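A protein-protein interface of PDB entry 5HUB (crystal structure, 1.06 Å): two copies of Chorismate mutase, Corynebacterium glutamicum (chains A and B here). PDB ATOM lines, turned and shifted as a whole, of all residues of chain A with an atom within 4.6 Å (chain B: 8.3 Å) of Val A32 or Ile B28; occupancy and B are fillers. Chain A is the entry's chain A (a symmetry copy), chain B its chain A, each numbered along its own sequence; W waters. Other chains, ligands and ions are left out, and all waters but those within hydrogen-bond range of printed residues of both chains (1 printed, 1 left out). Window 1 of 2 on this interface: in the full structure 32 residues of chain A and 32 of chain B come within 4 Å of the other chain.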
ATOM      1  N   ILE A  28      -1.835 -19.991 -17.228  1.00  0.00           N
ATOM      2  CA  ILE A  28      -1.931 -18.813 -18.097  1.00  0.00           C
ATOM      3  C   ILE A  28      -3.339 -18.642 -18.544  1.00  0.00           C
ATOM      4  O   ILE A  28      -3.875 -17.473 -18.402  1.00  0.00           O
ATOM      5  CB  ILE A  28      -0.980 -18.968 -19.306  1.00  0.00           C
ATOM      6  CG1 ILE A  28       0.456 -18.908 -18.865  1.00  0.00           C
ATOM      7  CG2 ILE A  28      -1.303 -17.931 -20.381  1.00  0.00           C
ATOM      8  CD1 ILE A  28       1.469 -19.418 -19.905  1.00  0.00           C
ATOM      9  N   LEU A  29      -4.029 -19.664 -19.025  1.00  0.00           N
ATOM     10  CA  LEU A  29      -5.397 -19.552 -19.456  1.00  0.00           C
ATOM     11  C   LEU A  29      -6.320 -19.127 -18.296  1.00  0.00           C
ATOM     12  O   LEU A  29      -7.201 -18.236 -18.495  1.00  0.00           O
ATOM     13  CB  LEU A  29      -5.885 -20.804 -20.112  1.00  0.00           C
ATOM     14  CG  LEU A  29      -5.265 -21.060 -21.492  1.00  0.00           C
ATOM     15  CD1 LEU A  29      -5.404 -22.511 -21.892  1.00  0.00           C
ATOM     16  CD2 LEU A  29      -5.889 -20.168 -22.544  1.00  0.00           C
ATOM     17  N   ASP A  30      -6.134 -19.682 -17.128  1.00  0.00           N
ATOM     18  CA  ASP A  30      -6.946 -19.314 -15.950  1.00  0.00           C
ATOM     19  C   ASP A  30      -6.787 -17.803 -15.672  1.00  0.00           C
ATOM     20  O   ASP A  30      -7.786 -17.108 -15.361  1.00  0.00           O
ATOM     21  CB  ASP A  30      -6.489 -20.112 -14.702  1.00  0.00           C
ATOM     22  CG  ASP A  30      -6.950 -21.554 -14.672  1.00  0.00           C
ATOM     23  OD1 ASP A  30      -7.830 -21.898 -15.459  1.00  0.00           O
ATOM     24  OD2 ASP A  30      -6.461 -22.329 -13.802  1.00  0.00           O
ATOM     25  N   ALA A  31      -5.582 -17.322 -15.629  1.00  0.00           N
ATOM     26  CA  ALA A  31      -5.320 -15.907 -15.320  1.00  0.00           C
ATOM     27  C   ALA A  31      -5.829 -15.049 -16.450  1.00  0.00           C
ATOM     28  O   ALA A  31      -6.359 -13.912 -16.128  1.00  0.00           O
ATOM     29  CB  ALA A  31      -3.854 -15.694 -15.069  1.00  0.00           C
ATOM     30  N   VAL A  32      -5.643 -15.355 -17.713  1.00  0.00           N
ATOM     31  CA  VAL A  32      -6.228 -14.598 -18.778  1.00  0.00           C
ATOM     32  C   VAL A  32      -7.746 -14.535 -18.715  1.00  0.00           C
ATOM     33  O   VAL A  32      -8.333 -13.415 -18.880  1.00  0.00           O
ATOM     34  CB  VAL A  32      -5.748 -15.192 -20.156  1.00  0.00           C
ATOM     35  CG1 VAL A  32      -6.539 -14.576 -21.287  1.00  0.00           C
ATOM     36  CG2 VAL A  32      -4.258 -15.005 -20.284  1.00  0.00           C
ATOM     37  N   LYS A  33      -8.419 -15.614 -18.374  1.00  0.00           N
ATOM     38  CA  LYS A  33      -9.856 -15.598 -18.233  1.00  0.00           C
ATOM     39  C   LYS A  33     -10.266 -14.641 -17.068  1.00  0.00           C
ATOM     40  O   LYS A  33     -11.231 -13.851 -17.205  1.00  0.00           O
ATOM     41  CB  LYS A  33     -10.379 -16.991 -17.989  1.00  0.00           C
ATOM     42  CG  LYS A  33     -10.265 -17.892 -19.198  1.00  0.00           C
ATOM     43  CD  LYS A  33     -10.812 -19.290 -18.844  1.00  0.00           C
ATOM     44  CE  LYS A  33     -10.472 -20.339 -19.835  1.00  0.00           C
ATOM     45  NZ  LYS A  33     -11.149 -21.616 -19.499  1.00  0.00           N
ATOM     46  N   ARG A  34      -9.597 -14.773 -15.937  1.00  0.00           N
ATOM     47  CA  ARG A  34      -9.918 -13.924 -14.772  1.00  0.00           C
ATOM     48  C   ARG A  34      -9.682 -12.464 -15.123  1.00  0.00           C
ATOM     49  O   ARG A  34     -10.556 -11.589 -14.806  1.00  0.00           O
ATOM     50  CB  ARG A  34      -9.065 -14.311 -13.583  1.00  0.00           C
ATOM     51  CG  ARG A  34      -9.560 -15.508 -12.784  1.00  0.00           C
ATOM     52  CD  ARG A  34      -8.741 -15.766 -11.531  1.00  0.00           C
ATOM     53  NE  ARG A  34      -7.515 -16.469 -11.840  1.00  0.00           N
ATOM     54  CZ  ARG A  34      -6.327 -16.128 -11.363  1.00  0.00           C
ATOM     55  NH1 ARG A  34      -6.217 -15.116 -10.531  1.00  0.00           N
ATOM     56  NH2 ARG A  34      -5.261 -16.802 -11.718  1.00  0.00           N
ATOM     57  N   ARG A  35      -8.567 -12.113 -15.715  1.00  0.00           N
ATOM     58  CA  ARG A  35      -8.248 -10.714 -16.121  1.00  0.00           C
ATOM     59  C   ARG A  35      -9.296 -10.204 -17.052  1.00  0.00           C
ATOM     60  O   ARG A  35      -9.747  -9.023 -16.849  1.00  0.00           O
ATOM     61  CB  ARG A  35      -6.879 -10.762 -16.866  1.00  0.00           C
ATOM     62  CG  ARG A  35      -6.315  -9.359 -17.079  1.00  0.00           C
ATOM     63  CD  ARG A  35      -5.431  -9.360 -18.299  1.00  0.00           C
ATOM     64  NE  ARG A  35      -4.651  -8.152 -18.359  1.00  0.00           N
ATOM     65  CZ  ARG A  35      -5.109  -6.979 -18.791  1.00  0.00           C
ATOM     66  NH1 ARG A  35      -4.321  -5.910 -18.689  1.00  0.00           N
ATOM     67  NH2 ARG A  35      -6.324  -6.885 -19.300  1.00  0.00           N
ATOM     68  N   THR A  36      -9.766 -10.994 -17.996  1.00  0.00           N
ATOM     69  CA  THR A  36     -10.673 -10.515 -19.014  1.00  0.00           C
ATOM     70  C   THR A  36     -12.041 -10.307 -18.394  1.00  0.00           C
ATOM     71  O   THR A  36     -12.659  -9.278 -18.635  1.00  0.00           O
ATOM     72  CB  THR A  36     -10.693 -11.517 -20.149  1.00  0.00           C
ATOM     73  OG1 THR A  36      -9.373 -11.568 -20.739  1.00  0.00           O
ATOM     74  CG2 THR A  36     -11.720 -11.184 -21.169  1.00  0.00           C
ATOM     75  N   LEU A  81      -4.500  -9.036 -24.670  1.00  0.00           N
ATOM     76  CA  LEU A  81      -5.173  -8.895 -23.392  1.00  0.00           C
ATOM     77  C   LEU A  81      -6.062  -7.625 -23.418  1.00  0.00           C
ATOM     78  O   LEU A  81      -7.164  -7.613 -22.916  1.00  0.00           O
ATOM     79  CB  LEU A  81      -4.169  -8.835 -22.275  1.00  0.00           C
ATOM     80  CG  LEU A  81      -3.334 -10.088 -22.082  1.00  0.00           C
ATOM     81  CD1 LEU A  81      -2.326  -9.894 -20.965  1.00  0.00           C
ATOM     82  CD2 LEU A  81      -4.199 -11.307 -21.884  1.00  0.00           C
ATOM     83  N   MET A  84      -9.149  -8.310 -25.609  1.00  0.00           N
ATOM     84  CA  MET A  84     -10.062  -9.142 -24.856  1.00  0.00           C
ATOM     85  C   MET A  84     -10.821  -8.407 -23.746  1.00  0.00           C
ATOM     86  O   MET A  84     -12.002  -8.699 -23.470  1.00  0.00           O
ATOM     87  CB  MET A  84      -9.304 -10.290 -24.238  1.00  0.00           C
ATOM     88  CG  MET A  84      -8.828 -11.337 -25.245  1.00  0.00           C
ATOM     89  SD  MET A  84      -7.906 -12.692 -24.502  1.00  0.00           S
ATOM     90  CE  MET A  84      -9.266 -13.566 -23.757  1.00  0.00           C
ATOM     91  N   GLU B  20      -6.236  -5.658  -8.932  1.00  0.00           N
ATOM     92  CA  GLU B  20      -6.244  -7.102  -9.260  1.00  0.00           C
ATOM     93  C   GLU B  20      -5.732  -7.307 -10.655  1.00  0.00           C
ATOM     94  O   GLU B  20      -4.995  -8.322 -10.886  1.00  0.00           O
ATOM     95  CB  GLU B  20      -7.641  -7.637  -9.140  1.00  0.00           C
ATOM     96  CG  GLU B  20      -7.533  -9.162  -9.086  1.00  0.00           C
ATOM     97  CD  GLU B  20      -8.751  -9.952  -8.695  1.00  0.00           C
ATOM     98  OE1 GLU B  20      -9.767  -9.309  -8.366  1.00  0.00           O
ATOM     99  OE2 GLU B  20      -8.659 -11.187  -8.673  1.00  0.00           O
ATOM    100  N   ILE B  21      -6.089  -6.563 -11.660  1.00  0.00           N
ATOM    101  CA  ILE B  21      -5.522  -6.730 -13.012  1.00  0.00           C
ATOM    102  C   ILE B  21      -4.031  -6.538 -12.980  1.00  0.00           C
ATOM    103  O   ILE B  21      -3.328  -7.336 -13.644  1.00  0.00           O
ATOM    104  CB  ILE B  21      -6.242  -5.802 -14.018  1.00  0.00           C
ATOM    105  CG1 ILE B  21      -7.669  -6.248 -14.220  1.00  0.00           C
ATOM    106  CG2 ILE B  21      -5.474  -5.695 -15.326  1.00  0.00           C
ATOM    107  CD1 ILE B  21      -8.520  -5.204 -14.944  1.00  0.00           C
ATOM    108  N   ASN B  22      -3.471  -5.574 -12.243  1.00  0.00           N
ATOM    109  CA  ASN B  22      -2.028  -5.461 -12.092  1.00  0.00           C
ATOM    110  C   ASN B  22      -1.402  -6.795 -11.615  1.00  0.00           C
ATOM    111  O   ASN B  22      -0.368  -7.238 -12.128  1.00  0.00           O
ATOM    112  CB  ASN B  22      -1.674  -4.315 -11.087  1.00  0.00           C
ATOM    113  CG  ASN B  22      -2.008  -2.881 -11.585  1.00  0.00           C
ATOM    114  OD1 ASN B  22      -2.292  -2.651 -12.718  1.00  0.00           O
ATOM    115  ND2 ASN B  22      -2.000  -1.911 -10.643  1.00  0.00           N
ATOM    116  N   ARG B  23      -1.996  -7.339 -10.600  1.00  0.00           N
ATOM    117  CA  ARG B  23      -1.440  -8.592 -10.033  1.00  0.00           C
ATOM    118  C   ARG B  23      -1.632  -9.744 -11.026  1.00  0.00           C
ATOM    119  O   ARG B  23      -0.750 -10.639 -11.120  1.00  0.00           O
ATOM    120  CB  ARG B  23      -2.039  -8.886  -8.652  1.00  0.00           C
ATOM    121  CG  ARG B  23      -1.556  -7.970  -7.528  1.00  0.00           C
ATOM    122  CD  ARG B  23      -1.992  -8.515  -6.174  1.00  0.00           C
ATOM    123  NE  ARG B  23      -3.451  -8.522  -5.962  1.00  0.00           N
ATOM    124  CZ  ARG B  23      -4.146  -7.491  -5.475  1.00  0.00           C
ATOM    125  NH1 ARG B  23      -3.527  -6.362  -5.184  1.00  0.00           N
ATOM    126  NH2 ARG B  23      -5.448  -7.621  -5.299  1.00  0.00           N
ATOM    127  N   LEU B  24      -2.703  -9.806 -11.764  1.00  0.00           N
ATOM    128  CA  LEU B  24      -2.866 -10.869 -12.785  1.00  0.00           C
ATOM    129  C   LEU B  24      -1.876 -10.678 -13.870  1.00  0.00           C
ATOM    130  O   LEU B  24      -1.373 -11.747 -14.400  1.00  0.00           O
ATOM    131  CB  LEU B  24      -4.293 -10.842 -13.307  1.00  0.00           C
ATOM    132  CG  LEU B  24      -5.316 -11.407 -12.360  1.00  0.00           C
ATOM    133  CD1 LEU B  24      -6.741 -10.991 -12.669  1.00  0.00           C
ATOM    134  CD2 LEU B  24      -5.247 -12.924 -12.399  1.00  0.00           C
ATOM    135  N   ASP B  25      -1.528  -9.482 -14.290  1.00  0.00           N
ATOM    136  CA  ASP B  25      -0.508  -9.341 -15.351  1.00  0.00           C
ATOM    137  C   ASP B  25       0.818  -9.796 -14.837  1.00  0.00           C
ATOM    138  O   ASP B  25       1.572 -10.475 -15.587  1.00  0.00           O
ATOM    139  CB  ASP B  25      -0.498  -7.888 -15.845  1.00  0.00           C
ATOM    140  CG  ASP B  25      -1.635  -7.622 -16.761  1.00  0.00           C
ATOM    141  OD1 ASP B  25      -2.285  -8.551 -17.286  1.00  0.00           O
ATOM    142  OD2 ASP B  25      -1.888  -6.369 -16.989  1.00  0.00           O
ATOM    143  N   ARG B  26       1.142  -9.607 -13.594  1.00  0.00           N
ATOM    144  CA  ARG B  26       2.344 -10.159 -12.993  1.00  0.00           C
ATOM    145  C   ARG B  26       2.327 -11.698 -13.046  1.00  0.00           C
ATOM    146  O   ARG B  26       3.357 -12.321 -13.358  1.00  0.00           O
ATOM    147  CB  ARG B  26       2.491  -9.633 -11.549  1.00  0.00           C
ATOM    148  CG  ARG B  26       3.369 -10.379 -10.561  1.00  0.00           C
ATOM    149  CD  ARG B  26       4.803  -9.961 -10.640  1.00  0.00           C
ATOM    150  NE  ARG B  26       5.443 -10.598 -11.776  1.00  0.00           N
ATOM    151  CZ  ARG B  26       5.816  -9.974 -12.888  1.00  0.00           C
ATOM    152  NH1 ARG B  26       5.666  -8.653 -13.023  1.00  0.00           N
ATOM    153  NH2 ARG B  26       6.340 -10.675 -13.864  1.00  0.00           N
ATOM    154  N   GLU B  27       1.215 -12.285 -12.666  1.00  0.00           N
ATOM    155  CA  GLU B  27       1.141 -13.739 -12.720  1.00  0.00           C
ATOM    156  C   GLU B  27       1.221 -14.235 -14.131  1.00  0.00           C
ATOM    157  O   GLU B  27       1.840 -15.320 -14.372  1.00  0.00           O
ATOM    158  CB  GLU B  27      -0.129 -14.196 -12.097  1.00  0.00           C
ATOM    159  CG  GLU B  27      -0.111 -14.041 -10.582  1.00  0.00           C
ATOM    160  CD  GLU B  27      -1.344 -14.609  -9.929  1.00  0.00           C
ATOM    161  OE1 GLU B  27      -1.482 -14.393  -8.698  1.00  0.00           O
ATOM    162  OE2 GLU B  27      -2.229 -15.200 -10.610  1.00  0.00           O
ATOM    163  N   ILE B  28       0.587 -13.644 -15.099  1.00  0.00           N
ATOM    164  CA  ILE B  28       0.694 -14.065 -16.500  1.00  0.00           C
ATOM    165  C   ILE B  28       2.107 -13.939 -16.948  1.00  0.00           C
ATOM    166  O   ILE B  28       2.645 -14.960 -17.530  1.00  0.00           O
ATOM    167  CB  ILE B  28      -0.246 -13.213 -17.383  1.00  0.00           C
ATOM    168  CG1 ILE B  28      -1.685 -13.521 -17.080  1.00  0.00           C
ATOM    169  CG2 ILE B  28       0.091 -13.399 -18.862  1.00  0.00           C
ATOM    170  CD1 ILE B  28      -2.690 -12.486 -17.616  1.00  0.00           C
ATOM    171  N   LEU B  29       2.799 -12.835 -16.712  1.00  0.00           N
ATOM    172  CA  LEU B  29       4.171 -12.670 -17.112  1.00  0.00           C
ATOM    173  C   LEU B  29       5.085 -13.709 -16.430  1.00  0.00           C
ATOM    174  O   LEU B  29       5.970 -14.305 -17.115  1.00  0.00           O
ATOM    175  CB  LEU B  29       4.661 -11.276 -16.881  1.00  0.00           C
ATOM    176  CG  LEU B  29       4.054 -10.241 -17.837  1.00  0.00           C
ATOM    177  CD1 LEU B  29       4.192  -8.841 -17.285  1.00  0.00           C
ATOM    178  CD2 LEU B  29       4.690 -10.325 -19.207  1.00  0.00           C
ATOM    179  N   ASP B  30       4.886 -13.965 -15.164  1.00  0.00           N
ATOM    180  CA  ASP B  30       5.687 -14.968 -14.435  1.00  0.00           C
ATOM    181  C   ASP B  30       5.531 -16.344 -15.121  1.00  0.00           C
ATOM    182  O   ASP B  30       6.529 -17.089 -15.280  1.00  0.00           O
ATOM    183  CB  ASP B  30       5.216 -15.077 -12.962  1.00  0.00           C
ATOM    184  CG  ASP B  30       5.673 -13.944 -12.068  1.00  0.00           C
ATOM    185  OD1 ASP B  30       6.558 -13.198 -12.483  1.00  0.00           O
ATOM    186  OD2 ASP B  30       5.173 -13.844 -10.912  1.00  0.00           O
ATOM    187  N   ALA B  31       4.327 -16.750 -15.387  1.00  0.00           N
ATOM    188  CA  ALA B  31       4.067 -18.067 -15.990  1.00  0.00           C
ATOM    189  C   ALA B  31       4.589 -18.077 -17.405  1.00  0.00           C
ATOM    190  O   ALA B  31       5.119 -19.181 -17.824  1.00  0.00           O
ATOM    191  CB  ALA B  31       2.599 -18.383 -15.932  1.00  0.00           C
ATOM    192  N   VAL B  32       4.413 -17.074 -18.233  1.00  0.00           N
ATOM    193  CA  VAL B  32       5.011 -17.043 -19.534  1.00  0.00           C
ATOM    194  C   VAL B  32       6.529 -17.135 -19.507  1.00  0.00           C
ATOM    195  O   VAL B  32       7.121 -17.934 -20.306  1.00  0.00           O
ATOM    196  CB  VAL B  32       4.542 -15.739 -20.284  1.00  0.00           C
ATOM    197  CG1 VAL B  32       5.346 -15.555 -21.551  1.00  0.00           C
ATOM    198  CG2 VAL B  32       3.054 -15.806 -20.513  1.00  0.00           C
ATOM    199  N   LYS B  33       7.195 -16.479 -18.581  1.00  0.00           N
ATOM    200  CA  LYS B  33       8.630 -16.580 -18.464  1.00  0.00           C
ATOM    201  C   LYS B  33       9.032 -18.046 -18.102  1.00  0.00           C
ATOM    202  O   LYS B  33      10.002 -18.599 -18.676  1.00  0.00           O
ATOM    203  CB  LYS B  33       9.147 -15.614 -17.427  1.00  0.00           C
ATOM    204  CG  LYS B  33       9.041 -14.167 -17.855  1.00  0.00           C
ATOM    205  CD  LYS B  33       9.581 -13.263 -16.728  1.00  0.00           C
ATOM    206  CE  LYS B  33       9.247 -11.828 -16.894  1.00  0.00           C
ATOM    207  NZ  LYS B  33       9.916 -11.011 -15.853  1.00  0.00           N
ATOM    208  N   ARG B  34       8.352 -18.618 -17.125  1.00  0.00           N
ATOM    209  CA  ARG B  34       8.665 -19.997 -16.699  1.00  0.00           C
ATOM    210  C   ARG B  34       8.437 -20.953 -17.857  1.00  0.00           C
ATOM    211  O   ARG B  34       9.311 -21.846 -18.121  1.00  0.00           O
ATOM    212  CB  ARG B  34       7.800 -20.398 -15.523  1.00  0.00           C
ATOM    213  CG  ARG B  34       8.284 -19.922 -14.161  1.00  0.00           C
ATOM    214  CD  ARG B  34       7.452 -20.464 -13.012  1.00  0.00           C
ATOM    215  NE  ARG B  34       6.227 -19.713 -12.849  1.00  0.00           N
ATOM    216  CZ  ARG B  34       5.035 -20.267 -12.683  1.00  0.00           C
ATOM    217  NH1 ARG B  34       4.921 -21.575 -12.626  1.00  0.00           N
ATOM    218  NH2 ARG B  34       3.971 -19.512 -12.573  1.00  0.00           N
ATOM    219  N   ARG B  35       7.329 -20.875 -18.552  1.00  0.00           N
ATOM    220  CA  ARG B  35       7.018 -21.750 -19.720  1.00  0.00           C
ATOM    221  C   ARG B  35       8.077 -21.603 -20.761  1.00  0.00           C
ATOM    222  O   ARG B  35       8.530 -22.671 -21.303  1.00  0.00           O
ATOM    223  CB  ARG B  35       5.656 -21.260 -20.300  1.00  0.00           C
ATOM    224  CG  ARG B  35       5.098 -22.253 -21.318  1.00  0.00           C
ATOM    225  CD  ARG B  35       4.227 -21.518 -22.301  1.00  0.00           C
ATOM    226  NE  ARG B  35       3.451 -22.445 -23.081  1.00  0.00           N
ATOM    227  CZ  ARG B  35       3.916 -23.126 -24.126  1.00  0.00           C
ATOM    228  NH1 ARG B  35       3.131 -24.040 -24.694  1.00  0.00           N
ATOM    229  NH2 ARG B  35       5.136 -22.900 -24.578  1.00  0.00           N
ATOM    230  N   PHE B  66      -6.262 -23.394 -26.740  1.00  0.00           N
ATOM    231  CA  PHE B  66      -6.380 -21.934 -26.453  1.00  0.00           C
ATOM    232  C   PHE B  66      -7.629 -21.385 -27.135  1.00  0.00           C
ATOM    233  O   PHE B  66      -8.370 -20.592 -26.500  1.00  0.00           O
ATOM    234  CB  PHE B  66      -5.117 -21.227 -26.903  1.00  0.00           C
ATOM    235  CG  PHE B  66      -3.997 -21.269 -25.904  1.00  0.00           C
ATOM    236  CD1 PHE B  66      -3.437 -22.440 -25.481  1.00  0.00           C
ATOM    237  CD2 PHE B  66      -3.557 -20.099 -25.304  1.00  0.00           C
ATOM    238  CE1 PHE B  66      -2.423 -22.480 -24.566  1.00  0.00           C
ATOM    239  CE2 PHE B  66      -2.571 -20.128 -24.346  1.00  0.00           C
ATOM    240  CZ  PHE B  66      -1.993 -21.328 -23.980  1.00  0.00           C
ATOM    241  N   GLU B  69     -10.709 -22.414 -25.017  1.00  0.00           N
ATOM    242  CA  GLU B  69     -10.763 -21.797 -23.695  1.00  0.00           C
ATOM    243  C   GLU B  69     -11.029 -20.304 -23.706  1.00  0.00           C
ATOM    244  O   GLU B  69     -11.751 -19.822 -22.840  1.00  0.00           O
ATOM    245  CB  GLU B  69      -9.469 -22.099 -22.938  1.00  0.00           C
ATOM    246  CG  GLU B  69      -9.174 -23.580 -22.799  1.00  0.00           C
ATOM    247  CD  GLU B  69      -9.569 -24.166 -21.462  1.00  0.00           C
ATOM    248  OE1 GLU B  69     -10.716 -23.934 -21.009  1.00  0.00           O
ATOM    249  OE2 GLU B  69      -8.698 -24.832 -20.852  1.00  0.00           O
ATOM    250  N   ILE B  70     -10.430 -19.585 -24.652  1.00  0.00           N
ATOM    251  CA  ILE B  70     -10.582 -18.097 -24.626  1.00  0.00           C
ATOM    252  C   ILE B  70     -11.180 -17.564 -25.903  1.00  0.00           C
ATOM    253  O   ILE B  70     -11.441 -16.382 -25.930  1.00  0.00           O
ATOM    254  CB  ILE B  70      -9.281 -17.355 -24.283  1.00  0.00           C
ATOM    255  CG1 ILE B  70      -8.155 -17.555 -25.327  1.00  0.00           C
ATOM    256  CG2 ILE B  70      -8.822 -17.666 -22.886  1.00  0.00           C
ATOM    257  CD1 ILE B  70      -6.998 -16.596 -25.095  1.00  0.00           C
ATOM    258  N   GLU B  73      -9.018 -15.000 -29.829  1.00  0.00           N
ATOM    259  CA  GLU B  73      -7.622 -14.660 -29.637  1.00  0.00           C
ATOM    260  C   GLU B  73      -6.759 -15.839 -29.205  1.00  0.00           C
ATOM    261  O   GLU B  73      -5.535 -15.713 -29.114  1.00  0.00           O
ATOM    262  CB  GLU B  73      -7.486 -13.588 -28.549  1.00  0.00           C
ATOM    263  CG  GLU B  73      -8.287 -12.316 -28.821  1.00  0.00           C
ATOM    264  CD  GLU B  73      -7.682 -11.464 -29.892  1.00  0.00           C
ATOM    265  OE1 GLU B  73      -6.567 -11.703 -30.355  1.00  0.00           O
ATOM    266  OE2 GLU B  73      -8.314 -10.441 -30.192  1.00  0.00           O
ATOM    267  N   GLY B  74      -7.388 -16.997 -28.993  1.00  0.00           N
ATOM    268  CA  GLY B  74      -6.621 -18.155 -28.524  1.00  0.00           C
ATOM    269  C   GLY B  74      -5.466 -18.538 -29.446  1.00  0.00           C
ATOM    270  O   GLY B  74      -4.357 -18.714 -29.019  1.00  0.00           O
ATOM    271  N   LEU B  77      -2.558 -16.084 -29.171  1.00  0.00           N
ATOM    272  CA  LEU B  77      -1.859 -16.201 -27.927  1.00  0.00           C
ATOM    273  C   LEU B  77      -0.951 -17.474 -27.915  1.00  0.00           C
ATOM    274  O   LEU B  77       0.216 -17.425 -27.520  1.00  0.00           O
ATOM    275  CB  LEU B  77      -2.850 -16.226 -26.754  1.00  0.00           C
ATOM    276  CG  LEU B  77      -2.268 -16.545 -25.361  1.00  0.00           C
ATOM    277  CD1 LEU B  77      -1.179 -15.547 -24.993  1.00  0.00           C
ATOM    278  CD2 LEU B  77      -3.371 -16.533 -24.313  1.00  0.00           C
ATOM    279  N   LEU B  81       3.357 -17.952 -27.601  1.00  0.00           N
ATOM    280  CA  LEU B  81       4.018 -18.833 -26.657  1.00  0.00           C
ATOM    281  C   LEU B  81       4.911 -19.836 -27.431  1.00  0.00           C
ATOM    282  O   LEU B  81       6.008 -20.150 -27.026  1.00  0.00           O
ATOM    283  CB  LEU B  81       3.004 -19.548 -25.808  1.00  0.00           C
ATOM    284  CG  LEU B  81       2.163 -18.659 -24.910  1.00  0.00           C
ATOM    285  CD1 LEU B  81       1.144 -19.481 -24.143  1.00  0.00           C
ATOM    286  CD2 LEU B  81       3.022 -17.805 -24.012  1.00  0.00           C
HETATM  287  O   HOH W   1     -13.829 -21.312 -21.639  1.00  0.00           O
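The side-chain carboxylate (OE2) of Glu B27 is in salt-bridge range of the guanidinium group (NH2) of Arg A34, at 3.6 Å.
The guanidinium group (NE) of Arg A35 is in salt-bridge range of the side-chain carboxylate (OD1) of Asp B25 (2.6 Å).
The side-chain amino group (NZ) of Lys A33 lies within salt-bridge range of the side-chain carboxylate (OE1) of Glu B69, 2.8 Å away.
The backbone carbonyl oxygen (O) of Val A32 lies within hydrogen-bond range of the side-chain hydroxyl (OG1) of Thr A36 (2.8 Å).
Among the printed residues, merely in contact across the chains: Ile A28 with Ala B31 (3.7 Å), Ile A28 with Val B32 (3.99 Å), Leu A29 with Phe B66 (3.6 Å), Leu A29 with Ile B70 (3.9 Å), Ala A31 with Ile B28 (3.7 Å), Val A32 with Ile B28 (3.99 Å), Lys A33 with Ile B70 (3.97 Å), Arg A34 with Leu B24 (3.0 Å), Arg A35 with Ile B21 (3.6 Å), Arg A35 with Leu B24 (3.7 Å), Leu A81 with Asp B25 (3.9 Å), Met A84 with Ile B70 (3.8 Å) and Met A84 with Glu B73 (3.7 Å).
Of the printed residues of chain B, Leu A29 touches Phe B66 and Ile B70.
Of the printed residues of chain B, Ala A31 touches Ile B28.
Printed residues of chain B within 4 Å of Val A32: Ile B28.
Printed residues of chain A within 4 Å of Ile B28: Ala A31 and Val A32.
Arg B34 touches none of the printed residues of chain A.
Printed residues of chain A within 4 Å of Ile B70: Leu A29, Lys A33 and Met A84.
Of the 23 printed residues of chain B, 11 touch a printed residue of chain A.
Hydrophobic or aromatic side chains of chain B that line the printed part of chain A: Ile B21, Leu B24, Ile B28, Ala B31, Val B32, Phe B66 and Ile B70.
Of the 11 printed residues of chain A, 9 touch a printed residue of chain B.
Hydrophobic or aromatic side chains of chain A that line the printed part of chain B: Ile A28, Leu A29, Ala A31, Val A32, Leu A81 and Met A84.
Among the printed residues, Asp or Glu carboxylates within 4 Å of a Lys or Arg side-chain nitrogen of the other chain: Lys A33 with Glu B69 (2.8 Å), Arg A34 with Glu B27 (3.6 Å) and Arg A35 with Asp B25 (2.6 Å).
Ile A28 touches Ala B31, and with the chains exchanged Ala A31 touches Ile B28.
Ile A28 touches Val B32, and with the chains exchanged Val A32 touches Ile B28.
Positions printed for both chains: 28, 29, 30, 31, 32, 33, 34, 35 and 81.
Of the 16 pairs that touch across the chains among the printed residues, 4 have their exchanged pair printed and touching as well.
Water W1 bridges O of Glu B69 (2.8 Å) and NZ of Lys A33 (3.4 Å).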
